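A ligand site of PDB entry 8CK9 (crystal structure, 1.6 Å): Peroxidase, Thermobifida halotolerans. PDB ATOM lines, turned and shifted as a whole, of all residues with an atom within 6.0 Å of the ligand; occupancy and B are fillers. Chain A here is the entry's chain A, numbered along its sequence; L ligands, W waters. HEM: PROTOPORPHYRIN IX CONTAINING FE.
FE of the ligand is bound by NE2 of His 336, 2.1 Å away. O2A of the ligand sits at hydrogen-bond distance from N of Gly 241. An oxygen (O2A) of the ligand is in salt-bridge range of the guanidinium group (NH1) of Arg 352, 2.8 Å away. O1A of the ligand is in hydrogen-bond range of N of Ala 243 (2.9 Å). The backbone NH of Thr 242 sits close to an oxygen (O2A) of the ligand.
The backbone NH (N) of His 336 is in hydrogen-bond range of the backbone carbonyl oxygen (O) of Leu 299, 3.4 Å away. O of Arg 352 sits at hydrogen-bond distance from ND2 of Asn 244 (2.8 Å). The side-chain amide nitrogen of Asn 234 is in hydrogen-bond range of the side-chain amide oxygen of Gln 238. The backbone carbonyl oxygen of Arg 278 is in hydrogen-bond range of the backbone NH of Phe 373 (2.9 Å). O of Leu 299 is in hydrogen-bond range of N of Val 337 (3.0 Å). The backbone NH of Met 236 is in hydrogen-bond range of the side-chain amide oxygen of Asn 234 (2.9 Å). A ring nitrogen (ND1) of His 404 is in hydrogen-bond range of the guanidinium group (NE) of Arg 278, 2.9 Å away. N of Leu 371 sits at hydrogen-bond distance from O of Ile 280.
Asn 234 touches the ligand (ND2 to CMB, 3.6 Å). SD of Met 236 touches CMB of the ligand, at 3.9 Å. Gln 238 touches the ligand. Ile 239 touches the ligand. Asp 240 touches the ligand (C to O2A, 3.9 Å). Ile 280 touches the ligand (CG2 to CBB, 3.6 Å). Met 282 touches the ligand (CE to CMB, 3.7 Å). Leu 299 touches the ligand. Arg 301 touches the ligand (CD to CAA, 3.8 Å). Val 337 touches the ligand (CG1 to CAA, 3.9 Å). Ala 340 touches the ligand. Asn 341 touches the ligand (CA to O1D, 3.9 Å). Pro 342 touches the ligand. Leu 371 touches the ligand. Phe 373 touches the ligand. Phe 384 touches the ligand (CE1 to CBC, 3.5 Å). CG1 of Val 387 touches CAC of the ligand, at 3.9 Å. Gln 388 touches the ligand (OE1 to CBC, 3.4 Å). Leu 391 touches the ligand. Leu 398 touches the ligand (CD2 to C2B, 3.5 Å). Thr 402 touches the ligand. His 404 touches the ligand (CE1 to CMC, 3.6 Å). Hydrophobic or aromatic side chains that line the ligand: Met 236, Ala 243, Ile 280, Met 282, Leu 299, His 336, Val 337, Ala 340, Pro 342, Leu 371, Phe 373, Phe 384, Val 387, Leu 391, Leu 398 and His 404. Of the 33 residues printed, 27 come within 4 Å of the ligand. The nearest printed residue that does not touch the ligand is Met 350 (4.1 Å).
Water W6 lies within hydrogen-bond range of an oxygen (O2D) of the ligand, the side-chain amide nitrogen (ND2) of Asn 341 and the backbone carbonyl oxygen (O) of Val 337. Water W7 bridges O2D of the ligand (2.7 Å) and NH2 of Arg 301 (3.2 Å). Water W2 lies within hydrogen-bond range of an oxygen (O2D) of the ligand (2.8 Å) and the guanidinium group (NE) of Arg 301 (2.8 Å). Water W4 lies within hydrogen-bond range of O1D of the ligand (2.9 Å) and O of Ala 243 (3.3 Å).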
ATOM      1  N   ASN A 234      24.787  24.403  -2.843  1.00  0.00           N
ATOM      2  CA  ASN A 234      25.023  23.449  -3.911  1.00  0.00           C
ATOM      3  C   ASN A 234      26.462  23.582  -4.401  1.00  0.00           C
ATOM      4  O   ASN A 234      27.256  24.347  -3.846  1.00  0.00           O
ATOM      5  CB  ASN A 234      24.003  23.638  -5.048  1.00  0.00           C
ATOM      6  CG  ASN A 234      24.091  25.025  -5.703  1.00  0.00           C
ATOM      7  OD1 ASN A 234      25.147  25.661  -5.714  1.00  0.00           O
ATOM      8  ND2 ASN A 234      22.977  25.475  -6.268  1.00  0.00           N
ATOM      9  N   MET A 236      27.644  24.919  -7.027  1.00  0.00           N
ATOM     10  CA  MET A 236      27.960  26.247  -7.526  1.00  0.00           C
ATOM     11  C   MET A 236      28.179  27.246  -6.396  1.00  0.00           C
ATOM     12  O   MET A 236      28.455  28.418  -6.682  1.00  0.00           O
ATOM     13  CB  MET A 236      26.835  26.741  -8.443  1.00  0.00           C
ATOM     14  CG  MET A 236      26.969  26.242  -9.873  1.00  0.00           C
ATOM     15  SD  MET A 236      25.451  26.544 -10.800  1.00  0.00           S
ATOM     16  CE  MET A 236      25.980  26.189 -12.468  1.00  0.00           C
ATOM     17  N   GLN A 238      25.896  28.179  -4.207  1.00  0.00           N
ATOM     18  CA  GLN A 238      24.695  28.969  -3.981  1.00  0.00           C
ATOM     19  C   GLN A 238      23.870  28.396  -2.842  1.00  0.00           C
ATOM     20  O   GLN A 238      23.757  27.185  -2.685  1.00  0.00           O
ATOM     21  CB  GLN A 238      23.831  28.992  -5.251  1.00  0.00           C
ATOM     22  CG  GLN A 238      24.520  29.496  -6.509  1.00  0.00           C
ATOM     23  CD  GLN A 238      23.822  29.058  -7.776  1.00  0.00           C
ATOM     24  OE1 GLN A 238      23.261  27.958  -7.856  1.00  0.00           O
ATOM     25  NE2 GLN A 238      23.856  29.923  -8.800  1.00  0.00           N
ATOM     26  N   ILE A 239      23.266  29.286  -2.052  1.00  0.00           N
ATOM     27  CA  ILE A 239      22.305  28.857  -1.055  1.00  0.00           C
ATOM     28  C   ILE A 239      21.088  28.303  -1.769  1.00  0.00           C
ATOM     29  O   ILE A 239      20.554  28.926  -2.689  1.00  0.00           O
ATOM     30  CB  ILE A 239      21.936  30.029  -0.131  1.00  0.00           C
ATOM     31  CG1 ILE A 239      23.151  30.421   0.707  1.00  0.00           C
ATOM     32  CG2 ILE A 239      20.776  29.654   0.756  1.00  0.00           C
ATOM     33  CD1 ILE A 239      22.972  31.722   1.462  1.00  0.00           C
ATOM     34  N   ASP A 240      20.655  27.111  -1.376  1.00  0.00           N
ATOM     35  CA  ASP A 240      19.742  26.299  -2.181  1.00  0.00           C
ATOM     36  C   ASP A 240      18.591  25.830  -1.295  1.00  0.00           C
ATOM     37  O   ASP A 240      18.765  24.928  -0.470  1.00  0.00           O
ATOM     38  CB  ASP A 240      20.514  25.113  -2.787  1.00  0.00           C
ATOM     39  CG  ASP A 240      19.652  24.215  -3.643  1.00  0.00           C
ATOM     40  OD1 ASP A 240      18.419  24.362  -3.641  1.00  0.00           O
ATOM     41  OD2 ASP A 240      20.237  23.338  -4.322  1.00  0.00           O
ATOM     42  N   GLY A 241      17.398  26.414  -1.488  1.00  0.00           N
ATOM     43  CA  GLY A 241      16.201  25.946  -0.817  1.00  0.00           C
ATOM     44  C   GLY A 241      15.337  27.035  -0.199  1.00  0.00           C
ATOM     45  O   GLY A 241      14.260  26.758   0.350  1.00  0.00           O
ATOM     46  N   THR A 242      15.794  28.283  -0.291  1.00  0.00           N
ATOM     47  CA  THR A 242      15.164  29.390   0.427  1.00  0.00           C
ATOM     48  C   THR A 242      13.660  29.491   0.186  1.00  0.00           C
ATOM     49  O   THR A 242      12.874  29.668   1.127  1.00  0.00           O
ATOM     50  CB  THR A 242      15.858  30.687   0.038  1.00  0.00           C
ATOM     51  OG1 THR A 242      17.250  30.555   0.341  1.00  0.00           O
ATOM     52  CG2 THR A 242      15.278  31.866   0.802  1.00  0.00           C
ATOM     53  N   ALA A 243      13.229  29.401  -1.080  1.00  0.00           N
ATOM     54  CA  ALA A 243      11.845  29.681  -1.418  1.00  0.00           C
ATOM     55  C   ALA A 243      10.915  28.487  -1.274  1.00  0.00           C
ATOM     56  O   ALA A 243       9.726  28.611  -1.586  1.00  0.00           O
ATOM     57  CB  ALA A 243      11.744  30.239  -2.844  1.00  0.00           C
ATOM     58  N   ASN A 244      11.408  27.354  -0.788  1.00  0.00           N
ATOM     59  CA  ASN A 244      10.526  26.218  -0.541  1.00  0.00           C
ATOM     60  C   ASN A 244       9.416  26.594   0.443  1.00  0.00           C
ATOM     61  O   ASN A 244       9.649  27.374   1.380  1.00  0.00           O
ATOM     62  CB  ASN A 244      11.307  25.045   0.049  1.00  0.00           C
ATOM     63  CG  ASN A 244      11.889  24.150  -1.015  1.00  0.00           C
ATOM     64  OD1 ASN A 244      11.301  23.997  -2.077  1.00  0.00           O
ATOM     65  ND2 ASN A 244      13.037  23.559  -0.739  1.00  0.00           N
ATOM     66  N   ARG A 278      15.456  15.188 -12.074  1.00  0.00           N
ATOM     67  CA  ARG A 278      16.275  15.617 -13.201  1.00  0.00           C
ATOM     68  C   ARG A 278      17.739  15.526 -12.819  1.00  0.00           C
ATOM     69  O   ARG A 278      18.143  16.013 -11.753  1.00  0.00           O
ATOM     70  CB  ARG A 278      15.941  17.061 -13.642  1.00  0.00           C
ATOM     71  CG  ARG A 278      14.476  17.273 -14.040  1.00  0.00           C
ATOM     72  CD  ARG A 278      14.125  16.652 -15.406  1.00  0.00           C
ATOM     73  NE  ARG A 278      14.592  17.479 -16.523  1.00  0.00           N
ATOM     74  CZ  ARG A 278      14.038  17.474 -17.723  1.00  0.00           C
ATOM     75  NH1 ARG A 278      13.054  16.627 -18.028  1.00  0.00           N
ATOM     76  NH2 ARG A 278      14.468  18.339 -18.645  1.00  0.00           N
ATOM     77  N   ILE A 280      21.006  17.020 -13.576  1.00  0.00           N
ATOM     78  CA  ILE A 280      21.397  18.281 -14.205  1.00  0.00           C
ATOM     79  C   ILE A 280      22.894  18.484 -13.996  1.00  0.00           C
ATOM     80  O   ILE A 280      23.329  18.838 -12.896  1.00  0.00           O
ATOM     81  CB  ILE A 280      20.608  19.486 -13.669  1.00  0.00           C
ATOM     82  CG1 ILE A 280      19.095  19.209 -13.677  1.00  0.00           C
ATOM     83  CG2 ILE A 280      20.954  20.723 -14.494  1.00  0.00           C
ATOM     84  CD1 ILE A 280      18.256  20.318 -13.001  1.00  0.00           C
ATOM     85  N   ARG A 281      23.667  18.317 -15.067  1.00  0.00           N
ATOM     86  CA  ARG A 281      25.109  18.533 -14.973  1.00  0.00           C
ATOM     87  C   ARG A 281      25.379  20.033 -14.888  1.00  0.00           C
ATOM     88  O   ARG A 281      24.764  20.823 -15.594  1.00  0.00           O
ATOM     89  CB  ARG A 281      25.804  17.918 -16.175  1.00  0.00           C
ATOM     90  CG  ARG A 281      27.309  18.064 -16.148  1.00  0.00           C
ATOM     91  CD  ARG A 281      27.961  17.176 -17.206  1.00  0.00           C
ATOM     92  NE  ARG A 281      27.526  17.500 -18.559  1.00  0.00           N
ATOM     93  CZ  ARG A 281      28.093  18.408 -19.345  1.00  0.00           C
ATOM     94  NH1 ARG A 281      29.110  19.139 -18.916  1.00  0.00           N
ATOM     95  NH2 ARG A 281      27.634  18.591 -20.573  1.00  0.00           N
ATOM     96  N   MET A 282      26.279  20.410 -13.992  1.00  0.00           N
ATOM     97  CA  MET A 282      26.729  21.797 -13.876  1.00  0.00           C
ATOM     98  C   MET A 282      28.030  21.981 -14.637  1.00  0.00           C
ATOM     99  O   MET A 282      28.941  21.148 -14.530  1.00  0.00           O
ATOM    100  CB  MET A 282      26.935  22.193 -12.422  1.00  0.00           C
ATOM    101  CG  MET A 282      25.662  22.292 -11.609  1.00  0.00           C
ATOM    102  SD  MET A 282      26.096  22.325  -9.863  1.00  0.00           S
ATOM    103  CE  MET A 282      24.607  23.029  -9.112  1.00  0.00           C
ATOM    104  N   LEU A 299      21.745  34.287 -11.073  1.00  0.00           N
ATOM    105  CA  LEU A 299      20.767  33.689 -10.171  1.00  0.00           C
ATOM    106  C   LEU A 299      19.666  34.664  -9.752  1.00  0.00           C
ATOM    107  O   LEU A 299      18.482  34.324  -9.772  1.00  0.00           O
ATOM    108  CB  LEU A 299      21.475  33.127  -8.938  1.00  0.00           C
ATOM    109  CG  LEU A 299      20.572  32.487  -7.890  1.00  0.00           C
ATOM    110  CD1 LEU A 299      19.927  31.228  -8.445  1.00  0.00           C
ATOM    111  CD2 LEU A 299      21.355  32.170  -6.632  1.00  0.00           C
ATOM    112  N   ARG A 301      20.106  36.159  -6.630  1.00  0.00           N
ATOM    113  CA  ARG A 301      20.337  36.205  -5.191  1.00  0.00           C
ATOM    114  C   ARG A 301      21.836  36.245  -4.931  1.00  0.00           C
ATOM    115  O   ARG A 301      22.640  35.795  -5.743  1.00  0.00           O
ATOM    116  CB  ARG A 301      19.715  34.983  -4.481  1.00  0.00           C
ATOM    117  CG  ARG A 301      18.196  35.016  -4.408  1.00  0.00           C
ATOM    118  CD  ARG A 301      17.668  33.769  -3.703  1.00  0.00           C
ATOM    119  NE  ARG A 301      16.228  33.784  -3.438  1.00  0.00           N
ATOM    120  CZ  ARG A 301      15.675  34.246  -2.321  1.00  0.00           C
ATOM    121  NH1 ARG A 301      16.397  34.888  -1.409  1.00  0.00           N
ATOM    122  NH2 ARG A 301      14.379  34.083  -2.123  1.00  0.00           N
ATOM    123  N   VAL A 318      11.761  38.419  -2.942  1.00  0.00           N
ATOM    124  CA  VAL A 318      12.211  38.758  -4.298  1.00  0.00           C
ATOM    125  C   VAL A 318      11.153  39.677  -4.888  1.00  0.00           C
ATOM    126  O   VAL A 318      10.021  39.262  -5.122  1.00  0.00           O
ATOM    127  CB  VAL A 318      12.403  37.497  -5.159  1.00  0.00           C
ATOM    128  CG1 VAL A 318      12.890  37.891  -6.549  1.00  0.00           C
ATOM    129  CG2 VAL A 318      13.390  36.539  -4.511  1.00  0.00           C
ATOM    130  N   HIS A 336      17.465  33.392 -12.905  1.00  0.00           N
ATOM    131  CA  HIS A 336      16.791  32.139 -12.580  1.00  0.00           C
ATOM    132  C   HIS A 336      15.629  32.345 -11.622  1.00  0.00           C
ATOM    133  O   HIS A 336      14.539  31.794 -11.830  1.00  0.00           O
ATOM    134  CB  HIS A 336      17.812  31.171 -11.968  1.00  0.00           C
ATOM    135  CG  HIS A 336      17.244  29.836 -11.597  1.00  0.00           C
ATOM    136  ND1 HIS A 336      16.824  28.906 -12.526  1.00  0.00           N
ATOM    137  CD2 HIS A 336      17.067  29.275 -10.376  1.00  0.00           C
ATOM    138  CE1 HIS A 336      16.405  27.824 -11.893  1.00  0.00           C
ATOM    139  NE2 HIS A 336      16.540  28.018 -10.593  1.00  0.00           N
ATOM    140  N   VAL A 337      15.844  33.106 -10.544  1.00  0.00           N
ATOM    141  CA  VAL A 337      14.762  33.192  -9.551  1.00  0.00           C
ATOM    142  C   VAL A 337      13.597  34.024 -10.061  1.00  0.00           C
ATOM    143  O   VAL A 337      12.480  33.878  -9.556  1.00  0.00           O
ATOM    144  CB  VAL A 337      15.264  33.724  -8.205  1.00  0.00           C
ATOM    145  CG1 VAL A 337      16.410  32.862  -7.656  1.00  0.00           C
ATOM    146  CG2 VAL A 337      15.656  35.210  -8.262  1.00  0.00           C
ATOM    147  N   ALA A 340      11.731  31.269 -12.435  1.00  0.00           N
ATOM    148  CA  ALA A 340      11.229  30.126 -11.675  1.00  0.00           C
ATOM    149  C   ALA A 340      10.147  30.504 -10.657  1.00  0.00           C
ATOM    150  O   ALA A 340       9.475  29.601 -10.126  1.00  0.00           O
ATOM    151  CB  ALA A 340      12.377  29.426 -10.945  1.00  0.00           C
ATOM    152  N   ASN A 341       9.952  31.784 -10.392  1.00  0.00           N
ATOM    153  CA  ASN A 341       9.042  32.246  -9.352  1.00  0.00           C
ATOM    154  C   ASN A 341       7.603  31.854  -9.706  1.00  0.00           C
ATOM    155  O   ASN A 341       7.195  31.980 -10.859  1.00  0.00           O
ATOM    156  CB  ASN A 341       9.145  33.768  -9.227  1.00  0.00           C
ATOM    157  CG  ASN A 341       8.513  34.321  -7.967  1.00  0.00           C
ATOM    158  OD1 ASN A 341       7.309  34.253  -7.790  1.00  0.00           O
ATOM    159  ND2 ASN A 341       9.333  34.923  -7.107  1.00  0.00           N
ATOM    160  N   PRO A 342       6.806  31.412  -8.721  1.00  0.00           N
ATOM    161  CA  PRO A 342       5.377  31.179  -9.008  1.00  0.00           C
ATOM    162  C   PRO A 342       4.700  32.369  -9.667  1.00  0.00           C
ATOM    163  O   PRO A 342       3.832  32.154 -10.526  1.00  0.00           O
ATOM    164  CB  PRO A 342       4.801  30.872  -7.622  1.00  0.00           C
ATOM    165  CG  PRO A 342       5.964  30.234  -6.900  1.00  0.00           C
ATOM    166  CD  PRO A 342       7.178  31.003  -7.357  1.00  0.00           C
ATOM    167  N   MET A 350       6.441  24.135  -6.403  1.00  0.00           N
ATOM    168  CA  MET A 350       6.885  22.777  -6.083  1.00  0.00           C
ATOM    169  C   MET A 350       7.732  22.826  -4.816  1.00  0.00           C
ATOM    170  O   MET A 350       8.140  23.890  -4.351  1.00  0.00           O
ATOM    171  CB  MET A 350       7.669  22.151  -7.242  1.00  0.00           C
ATOM    172  CG  MET A 350       9.032  22.792  -7.477  1.00  0.00           C
ATOM    173  SD  MET A 350       9.619  22.691  -9.187  1.00  0.00           S
ATOM    174  CE  MET A 350       8.681  24.028  -9.917  1.00  0.00           C
ATOM    175  N   ARG A 352      11.249  21.535  -3.544  1.00  0.00           N
ATOM    176  CA  ARG A 352      12.520  21.045  -4.067  1.00  0.00           C
ATOM    177  C   ARG A 352      13.352  20.427  -2.940  1.00  0.00           C
ATOM    178  O   ARG A 352      13.664  21.084  -1.947  1.00  0.00           O
ATOM    179  CB  ARG A 352      13.269  22.190  -4.750  1.00  0.00           C
ATOM    180  CG  ARG A 352      12.540  22.671  -6.002  1.00  0.00           C
ATOM    181  CD  ARG A 352      12.988  24.069  -6.479  1.00  0.00           C
ATOM    182  NE  ARG A 352      12.660  25.088  -5.482  1.00  0.00           N
ATOM    183  CZ  ARG A 352      13.562  25.853  -4.886  1.00  0.00           C
ATOM    184  NH1 ARG A 352      14.826  25.837  -5.241  1.00  0.00           N
ATOM    185  NH2 ARG A 352      13.165  26.663  -3.904  1.00  0.00           N
ATOM    186  N   GLY A 370      26.941  17.731 -10.609  1.00  0.00           N
ATOM    187  CA  GLY A 370      25.859  18.680 -10.737  1.00  0.00           C
ATOM    188  C   GLY A 370      24.796  18.526  -9.678  1.00  0.00           C
ATOM    189  O   GLY A 370      25.083  18.193  -8.515  1.00  0.00           O
ATOM    190  N   LEU A 371      23.559  18.777 -10.077  1.00  0.00           N
ATOM    191  CA  LEU A 371      22.422  18.767  -9.175  1.00  0.00           C
ATOM    192  C   LEU A 371      21.545  17.565  -9.496  1.00  0.00           C
ATOM    193  O   LEU A 371      21.069  17.440 -10.629  1.00  0.00           O
ATOM    194  CB  LEU A 371      21.619  20.055  -9.297  1.00  0.00           C
ATOM    195  CG  LEU A 371      20.336  20.126  -8.435  1.00  0.00           C
ATOM    196  CD1 LEU A 371      20.662  20.092  -6.940  1.00  0.00           C
ATOM    197  CD2 LEU A 371      19.531  21.383  -8.789  1.00  0.00           C
ATOM    198  N   PHE A 373      18.326  17.011  -9.037  1.00  0.00           N
ATOM    199  CA  PHE A 373      17.116  17.790  -8.810  1.00  0.00           C
ATOM    200  C   PHE A 373      15.960  16.858  -8.516  1.00  0.00           C
ATOM    201  O   PHE A 373      15.732  15.888  -9.256  1.00  0.00           O
ATOM    202  CB  PHE A 373      16.855  18.635 -10.056  1.00  0.00           C
ATOM    203  CG  PHE A 373      15.527  19.339 -10.069  1.00  0.00           C
ATOM    204  CD1 PHE A 373      14.394  18.699 -10.548  1.00  0.00           C
ATOM    205  CD2 PHE A 373      15.419  20.658  -9.638  1.00  0.00           C
ATOM    206  CE1 PHE A 373      13.153  19.345 -10.565  1.00  0.00           C
ATOM    207  CE2 PHE A 373      14.188  21.321  -9.671  1.00  0.00           C
ATOM    208  CZ  PHE A 373      13.055  20.664 -10.134  1.00  0.00           C
ATOM    209  N   PHE A 384       6.374  21.361 -11.709  1.00  0.00           N
ATOM    210  CA  PHE A 384       7.592  21.302 -12.518  1.00  0.00           C
ATOM    211  C   PHE A 384       7.383  21.751 -13.962  1.00  0.00           C
ATOM    212  O   PHE A 384       8.191  22.506 -14.498  1.00  0.00           O
ATOM    213  CB  PHE A 384       8.144  19.879 -12.494  1.00  0.00           C
ATOM    214  CG  PHE A 384       9.304  19.672 -13.421  1.00  0.00           C
ATOM    215  CD1 PHE A 384      10.576  20.115 -13.067  1.00  0.00           C
ATOM    216  CD2 PHE A 384       9.125  19.063 -14.658  1.00  0.00           C
ATOM    217  CE1 PHE A 384      11.661  19.913 -13.929  1.00  0.00           C
ATOM    218  CE2 PHE A 384      10.208  18.870 -15.523  1.00  0.00           C
ATOM    219  CZ  PHE A 384      11.471  19.296 -15.154  1.00  0.00           C
ATOM    220  N   VAL A 387       7.043  25.588 -14.982  1.00  0.00           N
ATOM    221  CA  VAL A 387       8.256  26.285 -14.576  1.00  0.00           C
ATOM    222  C   VAL A 387       9.422  25.907 -15.480  1.00  0.00           C
ATOM    223  O   VAL A 387      10.155  26.768 -15.961  1.00  0.00           O
ATOM    224  CB  VAL A 387       8.555  26.026 -13.088  1.00  0.00           C
ATOM    225  CG1 VAL A 387       9.851  26.706 -12.689  1.00  0.00           C
ATOM    226  CG2 VAL A 387       7.397  26.567 -12.233  1.00  0.00           C
ATOM    227  N   GLN A 388       9.580  24.605 -15.774  1.00  0.00           N
ATOM    228  CA  GLN A 388      10.685  24.201 -16.645  1.00  0.00           C
ATOM    229  C   GLN A 388      10.503  24.757 -18.057  1.00  0.00           C
ATOM    230  O   GLN A 388      11.489  25.109 -18.712  1.00  0.00           O
ATOM    231  CB  GLN A 388      10.816  22.680 -16.663  1.00  0.00           C
ATOM    232  CG  GLN A 388      11.871  22.120 -17.616  1.00  0.00           C
ATOM    233  CD  GLN A 388      13.289  22.513 -17.253  1.00  0.00           C
ATOM    234  OE1 GLN A 388      13.541  23.135 -16.223  1.00  0.00           O
ATOM    235  NE2 GLN A 388      14.239  22.142 -18.117  1.00  0.00           N
ATOM    236  N   LEU A 391      11.854  28.283 -17.857  1.00  0.00           N
ATOM    237  CA  LEU A 391      13.310  28.317 -17.840  1.00  0.00           C
ATOM    238  C   LEU A 391      13.886  28.013 -19.226  1.00  0.00           C
ATOM    239  O   LEU A 391      14.828  28.669 -19.675  1.00  0.00           O
ATOM    240  CB  LEU A 391      13.843  27.320 -16.804  1.00  0.00           C
ATOM    241  CG  LEU A 391      13.335  27.515 -15.379  1.00  0.00           C
ATOM    242  CD1 LEU A 391      14.005  26.512 -14.432  1.00  0.00           C
ATOM    243  CD2 LEU A 391      13.585  28.942 -14.895  1.00  0.00           C
ATOM    244  N   LEU A 398      20.786  30.669 -16.235  1.00  0.00           N
ATOM    245  CA  LEU A 398      21.357  29.433 -15.730  1.00  0.00           C
ATOM    246  C   LEU A 398      21.444  28.352 -16.794  1.00  0.00           C
ATOM    247  O   LEU A 398      22.231  27.411 -16.634  1.00  0.00           O
ATOM    248  CB  LEU A 398      20.540  28.942 -14.531  1.00  0.00           C
ATOM    249  CG  LEU A 398      21.224  28.056 -13.515  1.00  0.00           C
ATOM    250  CD1 LEU A 398      22.605  28.586 -13.113  1.00  0.00           C
ATOM    251  CD2 LEU A 398      20.320  27.906 -12.283  1.00  0.00           C
ATOM    252  N   THR A 402      24.173  24.790 -17.268  1.00  0.00           N
ATOM    253  CA  THR A 402      23.564  23.539 -16.853  1.00  0.00           C
ATOM    254  C   THR A 402      23.110  22.737 -18.068  1.00  0.00           C
ATOM    255  O   THR A 402      22.823  23.303 -19.125  1.00  0.00           O
ATOM    256  CB  THR A 402      22.343  23.759 -15.936  1.00  0.00           C
ATOM    257  OG1 THR A 402      21.363  24.560 -16.619  1.00  0.00           O
ATOM    258  CG2 THR A 402      22.775  24.424 -14.650  1.00  0.00           C
ATOM    259  N   HIS A 404      20.471  19.318 -18.743  1.00  0.00           N
ATOM    260  CA  HIS A 404      19.574  18.269 -18.250  1.00  0.00           C
ATOM    261  C   HIS A 404      19.853  16.981 -19.021  1.00  0.00           C
ATOM    262  O   HIS A 404      19.568  16.905 -20.214  1.00  0.00           O
ATOM    263  CB  HIS A 404      18.115  18.673 -18.414  1.00  0.00           C
ATOM    264  CG  HIS A 404      17.694  19.767 -17.491  1.00  0.00           C
ATOM    265  ND1 HIS A 404      16.594  19.640 -16.665  1.00  0.00           N
ATOM    266  CD2 HIS A 404      18.212  20.997 -17.257  1.00  0.00           C
ATOM    267  CE1 HIS A 404      16.447  20.758 -15.966  1.00  0.00           C
ATOM    268  NE2 HIS A 404      17.415  21.589 -16.299  1.00  0.00           N
HETATM  269  CHA HEM L   1      15.393  28.864  -6.877  1.00  0.00           C
HETATM  270  CHB HEM L   1      19.624  26.860  -8.174  1.00  0.00           C
HETATM  271  CHC HEM L   1      17.344  24.188 -11.540  1.00  0.00           C
HETATM  272  CHD HEM L   1      13.095  25.759  -9.815  1.00  0.00           C
HETATM  273  C1A HEM L   1      16.737  28.540  -6.929  1.00  0.00           C
HETATM  274  C2A HEM L   1      17.763  29.108  -6.090  1.00  0.00           C
HETATM  275  C3A HEM L   1      18.931  28.536  -6.450  1.00  0.00           C
HETATM  276  C4A HEM L   1      18.671  27.615  -7.524  1.00  0.00           C
HETATM  277  CMA HEM L   1      20.347  28.797  -5.878  1.00  0.00           C
HETATM  278  CAA HEM L   1      17.543  30.188  -4.997  1.00  0.00           C
HETATM  279  CBA HEM L   1      17.329  29.656  -3.579  1.00  0.00           C
HETATM  280  CGA HEM L   1      16.016  28.927  -3.501  1.00  0.00           C
HETATM  281  O1A HEM L   1      14.955  29.605  -3.395  1.00  0.00           O
HETATM  282  O2A HEM L   1      16.032  27.674  -3.540  1.00  0.00           O
HETATM  283  C1B HEM L   1      19.376  26.010  -9.227  1.00  0.00           C
HETATM  284  C2B HEM L   1      20.375  25.263  -9.959  1.00  0.00           C
HETATM  285  C3B HEM L   1      19.744  24.536 -10.899  1.00  0.00           C
HETATM  286  C4B HEM L   1      18.322  24.774 -10.765  1.00  0.00           C
HETATM  287  CMB HEM L   1      21.884  25.394  -9.684  1.00  0.00           C
HETATM  288  CAB HEM L   1      20.323  23.545 -11.932  1.00  0.00           C
HETATM  289  CBB HEM L   1      21.448  22.878 -11.657  1.00  0.00           C
HETATM  290  C1C HEM L   1      15.993  24.375 -11.352  1.00  0.00           C
HETATM  291  C2C HEM L   1      14.939  23.721 -12.092  1.00  0.00           C
HETATM  292  C3C HEM L   1      13.758  24.141 -11.613  1.00  0.00           C
HETATM  293  C4C HEM L   1      14.047  25.097 -10.568  1.00  0.00           C
HETATM  294  CMC HEM L   1      15.186  22.688 -13.209  1.00  0.00           C
HETATM  295  CAC HEM L   1      12.311  23.780 -12.031  1.00  0.00           C
HETATM  296  CBC HEM L   1      11.962  23.335 -13.241  1.00  0.00           C
HETATM  297  C1D HEM L   1      13.361  26.714  -8.866  1.00  0.00           C
HETATM  298  C2D HEM L   1      12.363  27.421  -8.091  1.00  0.00           C
HETATM  299  C3D HEM L   1      12.969  28.285  -7.280  1.00  0.00           C
HETATM  300  C4D HEM L   1      14.398  28.150  -7.519  1.00  0.00           C
HETATM  301  CMD HEM L   1      10.844  27.189  -8.219  1.00  0.00           C
HETATM  302  CAD HEM L   1      12.313  29.249  -6.277  1.00  0.00           C
HETATM  303  CBD HEM L   1      11.881  30.537  -6.984  1.00  0.00           C
HETATM  304  CGD HEM L   1      11.174  31.421  -5.993  1.00  0.00           C
HETATM  305  O1D HEM L   1       9.972  31.164  -5.715  1.00  0.00           O
HETATM  306  O2D HEM L   1      11.810  32.376  -5.461  1.00  0.00           O
HETATM  307  NA  HEM L   1      17.318  27.624  -7.796  1.00  0.00           N
HETATM  308  NB  HEM L   1      18.144  25.678  -9.738  1.00  0.00           N
HETATM  309  NC  HEM L   1      15.415  25.218 -10.419  1.00  0.00           N
HETATM  310  ND  HEM L   1      14.598  27.184  -8.482  1.00  0.00           N
HETATM  311 FE   HEM L   1      16.384  26.506  -9.190  1.00  0.00          FE
HETATM  312  O   HOH W   1       8.051  26.630  -6.297  1.00  0.00           O
HETATM  313  O   HOH W   2      14.435  32.068  -4.656  1.00  0.00           O
HETATM  314  O   HOH W   3       7.638  27.788  -8.898  1.00  0.00           O
HETATM  315  O   HOH W   4       8.724  28.729  -4.698  1.00  0.00           O
HETATM  316  O   HOH W   5       8.261  32.074  -3.903  1.00  0.00           O
HETATM  317  O   HOH W   6      11.995  34.585  -6.963  1.00  0.00           O
HETATM  318  O   HOH W   7      11.348  33.737  -3.132  1.00  0.00           O
